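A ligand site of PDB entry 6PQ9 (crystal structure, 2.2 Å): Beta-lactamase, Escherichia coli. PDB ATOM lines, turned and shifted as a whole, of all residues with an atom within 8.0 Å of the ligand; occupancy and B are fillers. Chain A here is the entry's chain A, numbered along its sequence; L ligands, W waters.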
ATOM      1  N   LYS A  23      -3.146  20.124   9.116  1.00  0.00           N
ATOM      2  CA  LYS A  23      -2.490  19.231   8.170  1.00  0.00           C
ATOM      3  C   LYS A  23      -3.510  18.728   7.132  1.00  0.00           C
ATOM      4  O   LYS A  23      -4.730  18.804   7.360  1.00  0.00           O
ATOM      5  CB  LYS A  23      -1.814  18.064   8.907  1.00  0.00           C
ATOM      6  CG  LYS A  23      -0.389  17.705   8.459  1.00  0.00           C
ATOM      7  CD  LYS A  23      -0.343  17.014   7.111  1.00  0.00           C
ATOM      8  CE  LYS A  23       1.052  17.091   6.515  1.00  0.00           C
ATOM      9  NZ  LYS A  23       1.066  16.682   5.079  1.00  0.00           N
ATOM     10  N   GLY A  24      -3.027  18.243   5.992  1.00  0.00           N
ATOM     11  CA  GLY A  24      -3.895  17.729   4.954  1.00  0.00           C
ATOM     12  C   GLY A  24      -4.145  16.240   5.053  1.00  0.00           C
ATOM     13  O   GLY A  24      -5.205  15.758   4.633  1.00  0.00           O
ATOM     14  N   THR A  25      -3.187  15.496   5.612  1.00  0.00           N
ATOM     15  CA  THR A  25      -3.314  14.045   5.689  1.00  0.00           C
ATOM     16  C   THR A  25      -4.502  13.628   6.561  1.00  0.00           C
ATOM     17  O   THR A  25      -5.202  12.665   6.243  1.00  0.00           O
ATOM     18  CB  THR A  25      -2.026  13.420   6.208  1.00  0.00           C
ATOM     19  OG1 THR A  25      -0.902  14.023   5.550  1.00  0.00           O
ATOM     20  CG2 THR A  25      -2.012  11.906   5.932  1.00  0.00           C
ATOM     21  N   ASP A  52       9.273  10.049  -1.456  1.00  0.00           N
ATOM     22  CA  ASP A  52       9.197  10.766  -0.189  1.00  0.00           C
ATOM     23  C   ASP A  52       8.567   9.841   0.852  1.00  0.00           C
ATOM     24  O   ASP A  52       8.455   8.626   0.646  1.00  0.00           O
ATOM     25  CB  ASP A  52       8.455  12.091  -0.341  1.00  0.00           C
ATOM     26  CG  ASP A  52       7.011  11.929  -0.735  1.00  0.00           C
ATOM     27  OD1 ASP A  52       6.347  10.993  -0.247  1.00  0.00           O
ATOM     28  OD2 ASP A  52       6.520  12.764  -1.514  1.00  0.00           O
ATOM     29  N   PHE A  54       5.416  10.093   2.445  1.00  0.00           N
ATOM     30  CA  PHE A  54       3.977  10.164   2.648  1.00  0.00           C
ATOM     31  C   PHE A  54       3.422   8.812   3.102  1.00  0.00           C
ATOM     32  O   PHE A  54       3.783   7.754   2.571  1.00  0.00           O
ATOM     33  CB  PHE A  54       3.296  10.611   1.373  1.00  0.00           C
ATOM     34  CG  PHE A  54       1.832  10.749   1.513  1.00  0.00           C
ATOM     35  CD1 PHE A  54       1.285  11.903   2.013  1.00  0.00           C
ATOM     36  CD2 PHE A  54       0.990   9.683   1.211  1.00  0.00           C
ATOM     37  CE1 PHE A  54      -0.075  12.024   2.184  1.00  0.00           C
ATOM     38  CE2 PHE A  54      -0.370   9.784   1.369  1.00  0.00           C
ATOM     39  CZ  PHE A  54      -0.907  10.960   1.864  1.00  0.00           C
ATOM     40  N   LEU A 259       2.333   9.606 -10.564  1.00  0.00           N
ATOM     41  CA  LEU A 259       1.692  10.906 -10.483  1.00  0.00           C
ATOM     42  C   LEU A 259       2.068  11.742 -11.703  1.00  0.00           C
ATOM     43  O   LEU A 259       3.018  11.421 -12.419  1.00  0.00           O
ATOM     44  CB  LEU A 259       2.125  11.614  -9.210  1.00  0.00           C
ATOM     45  CG  LEU A 259       1.609  11.031  -7.889  1.00  0.00           C
ATOM     46  CD1 LEU A 259       2.637  11.267  -6.775  1.00  0.00           C
ATOM     47  CD2 LEU A 259       0.239  11.619  -7.512  1.00  0.00           C
ATOM     48  N   ASN A 261       3.669  14.464 -12.031  1.00  0.00           N
ATOM     49  CA  ASN A 261       5.031  14.980 -11.970  1.00  0.00           C
ATOM     50  C   ASN A 261       6.090  13.884 -12.125  1.00  0.00           C
ATOM     51  O   ASN A 261       7.287  14.184 -11.983  1.00  0.00           O
ATOM     52  CB  ASN A 261       5.266  15.706 -10.640  1.00  0.00           C
ATOM     53  CG  ASN A 261       5.157  14.770  -9.450  1.00  0.00           C
ATOM     54  OD1 ASN A 261       4.882  13.582  -9.592  1.00  0.00           O
ATOM     55  ND2 ASN A 261       5.389  15.307  -8.257  1.00  0.00           N
ATOM     56  N   LYS A 263       6.550  11.256 -10.120  1.00  0.00           N
ATOM     57  CA  LYS A 263       6.753  10.509  -8.892  1.00  0.00           C
ATOM     58  C   LYS A 263       5.702   9.402  -8.752  1.00  0.00           C
ATOM     59  O   LYS A 263       4.785   9.280  -9.568  1.00  0.00           O
ATOM     60  CB  LYS A 263       6.753  11.457  -7.706  1.00  0.00           C
ATOM     61  CG  LYS A 263       8.059  12.195  -7.537  1.00  0.00           C
ATOM     62  CD  LYS A 263       7.937  13.335  -6.554  1.00  0.00           C
ATOM     63  CE  LYS A 263       9.191  14.194  -6.534  1.00  0.00           C
ATOM     64  NZ  LYS A 263       9.001  15.342  -5.620  1.00  0.00           N
ATOM     65  N   VAL A 292      -6.980   9.876  -2.869  1.00  0.00           N
ATOM     66  CA  VAL A 292      -5.552   9.924  -2.576  1.00  0.00           C
ATOM     67  C   VAL A 292      -4.797  10.575  -3.730  1.00  0.00           C
ATOM     68  O   VAL A 292      -3.889  11.389  -3.524  1.00  0.00           O
ATOM     69  CB  VAL A 292      -5.018   8.510  -2.283  1.00  0.00           C
ATOM     70  CG1 VAL A 292      -3.493   8.497  -2.229  1.00  0.00           C
ATOM     71  CG2 VAL A 292      -5.650   7.949  -0.986  1.00  0.00           C
ATOM     72  N   TRP A 293      -5.192  10.257  -4.962  1.00  0.00           N
ATOM     73  CA  TRP A 293      -4.590  10.878  -6.144  1.00  0.00           C
ATOM     74  C   TRP A 293      -4.788  12.384  -6.125  1.00  0.00           C
ATOM     75  O   TRP A 293      -3.833  13.160  -6.307  1.00  0.00           O
ATOM     76  CB  TRP A 293      -5.206  10.233  -7.393  1.00  0.00           C
ATOM     77  CG  TRP A 293      -4.945  10.931  -8.677  1.00  0.00           C
ATOM     78  CD1 TRP A 293      -5.637  11.976  -9.209  1.00  0.00           C
ATOM     79  CD2 TRP A 293      -3.919  10.604  -9.626  1.00  0.00           C
ATOM     80  NE1 TRP A 293      -5.096  12.333 -10.429  1.00  0.00           N
ATOM     81  CE2 TRP A 293      -4.039  11.509 -10.702  1.00  0.00           C
ATOM     82  CE3 TRP A 293      -2.898   9.647  -9.672  1.00  0.00           C
ATOM     83  CZ2 TRP A 293      -3.185  11.474 -11.811  1.00  0.00           C
ATOM     84  CZ3 TRP A 293      -2.059   9.603 -10.768  1.00  0.00           C
ATOM     85  CH2 TRP A 293      -2.200  10.512 -11.820  1.00  0.00           C
ATOM     86  N   ASP A 294      -6.023  12.835  -5.874  1.00  0.00           N
ATOM     87  CA  ASP A 294      -6.348  14.260  -5.852  1.00  0.00           C
ATOM     88  C   ASP A 294      -5.514  14.992  -4.807  1.00  0.00           C
ATOM     89  O   ASP A 294      -4.956  16.054  -5.087  1.00  0.00           O
ATOM     90  CB  ASP A 294      -7.835  14.441  -5.548  1.00  0.00           C
ATOM     91  CG  ASP A 294      -8.701  14.173  -6.739  1.00  0.00           C
ATOM     92  OD1 ASP A 294      -8.157  13.938  -7.842  1.00  0.00           O
ATOM     93  OD2 ASP A 294      -9.948  14.202  -6.565  1.00  0.00           O
ATOM     94  N   TYR A 295      -5.445  14.443  -3.594  1.00  0.00           N
ATOM     95  CA  TYR A 295      -4.673  15.092  -2.535  1.00  0.00           C
ATOM     96  C   TYR A 295      -3.210  15.250  -2.915  1.00  0.00           C
ATOM     97  O   TYR A 295      -2.609  16.314  -2.718  1.00  0.00           O
ATOM     98  CB  TYR A 295      -4.819  14.294  -1.235  1.00  0.00           C
ATOM     99  CG  TYR A 295      -3.906  14.778  -0.131  1.00  0.00           C
ATOM    100  CD1 TYR A 295      -4.232  15.884   0.650  1.00  0.00           C
ATOM    101  CD2 TYR A 295      -2.698  14.139   0.117  1.00  0.00           C
ATOM    102  CE1 TYR A 295      -3.375  16.329   1.652  1.00  0.00           C
ATOM    103  CE2 TYR A 295      -1.852  14.570   1.111  1.00  0.00           C
ATOM    104  CZ  TYR A 295      -2.192  15.669   1.872  1.00  0.00           C
ATOM    105  OH  TYR A 295      -1.326  16.079   2.875  1.00  0.00           O
ATOM    106  N   LEU A 296      -2.592  14.198  -3.480  1.00  0.00           N
ATOM    107  CA  LEU A 296      -1.170  14.241  -3.792  1.00  0.00           C
ATOM    108  C   LEU A 296      -0.886  15.080  -5.037  1.00  0.00           C
ATOM    109  O   LEU A 296       0.203  15.661  -5.159  1.00  0.00           O
ATOM    110  CB  LEU A 296      -0.616  12.829  -3.976  1.00  0.00           C
ATOM    111  CG  LEU A 296      -0.673  11.880  -2.760  1.00  0.00           C
ATOM    112  CD1 LEU A 296      -0.255  10.453  -3.154  1.00  0.00           C
ATOM    113  CD2 LEU A 296       0.186  12.386  -1.615  1.00  0.00           C
ATOM    114  N   VAL A 297      -1.834  15.156  -5.972  1.00  0.00           N
ATOM    115  CA  VAL A 297      -1.675  16.063  -7.104  1.00  0.00           C
ATOM    116  C   VAL A 297      -1.656  17.506  -6.615  1.00  0.00           C
ATOM    117  O   VAL A 297      -0.822  18.307  -7.051  1.00  0.00           O
ATOM    118  CB  VAL A 297      -2.791  15.816  -8.141  1.00  0.00           C
ATOM    119  CG1 VAL A 297      -2.905  16.995  -9.092  1.00  0.00           C
ATOM    120  CG2 VAL A 297      -2.541  14.526  -8.904  1.00  0.00           C
ATOM    121  N   LYS A 298      -2.551  17.850  -5.685  1.00  0.00           N
ATOM    122  CA  LYS A 298      -2.685  19.216  -5.160  1.00  0.00           C
ATOM    123  C   LYS A 298      -1.468  19.661  -4.309  1.00  0.00           C
ATOM    124  O   LYS A 298      -1.166  20.849  -4.233  1.00  0.00           O
ATOM    125  CB  LYS A 298      -3.974  19.335  -4.338  1.00  0.00           C
ATOM    126  CG  LYS A 298      -4.259  20.721  -3.754  1.00  0.00           C
ATOM    127  CD  LYS A 298      -5.701  21.182  -4.020  1.00  0.00           C
ATOM    128  CE  LYS A 298      -6.708  20.376  -3.210  1.00  0.00           C
ATOM    129  NZ  LYS A 298      -8.068  21.026  -3.173  1.00  0.00           N
HETATM  130  N1  LIG L   1       1.374  18.340  -3.980  1.00  0.00           N
HETATM  131  C1  LIG L   1       2.424  18.350  -2.971  1.00  0.00           C
HETATM  132  C2  LIG L   1       3.112  16.968  -2.864  1.00  0.00           C
HETATM  133  O1  LIG L   1       4.320  16.874  -2.601  1.00  0.00           O
HETATM  134  C3  LIG L   1       1.852  18.762  -1.613  1.00  0.00           C
HETATM  135  C4  LIG L   1       0.933  17.700  -1.001  1.00  0.00           C
HETATM  136  O2  LIG L   1      -0.282  17.705  -1.323  1.00  0.00           O
HETATM  137  O3  LIG L   1       1.421  16.876  -0.188  1.00  0.00           O
HETATM  138  O   HOH W   1       6.135  16.427  -4.534  1.00  0.00           O
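An oxygen (O2) of the ligand sits close to the backbone carbonyl oxygen (O) of Tyr 295.
The backbone carbonyl oxygen of Leu 296 sits at hydrogen-bond distance from a nitrogen (N1) of the ligand (3.2 Å).
The side-chain hydroxyl (OH) of Tyr 295 lies within hydrogen-bond range of the side-chain amino group (NZ) of Lys 23 (3.3 Å).
The side-chain hydroxyl (OH) of Tyr 295 sits at hydrogen-bond distance from the backbone NH (N) of Thr 25 (3.4 Å).
Residues that only touch the ligand: Lys 298 (3.2 Å) and Val 297 (3.8 Å).
Within 4 Å of the ligand: Tyr 295, Leu 296, Val 297 and Lys 298.
Along chain A the residues within 4 Å of the ligand span positions 295 to 298.
Water W1 bridges an oxygen (O1) of the ligand and the side-chain amino group (NZ) of Lys 263.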
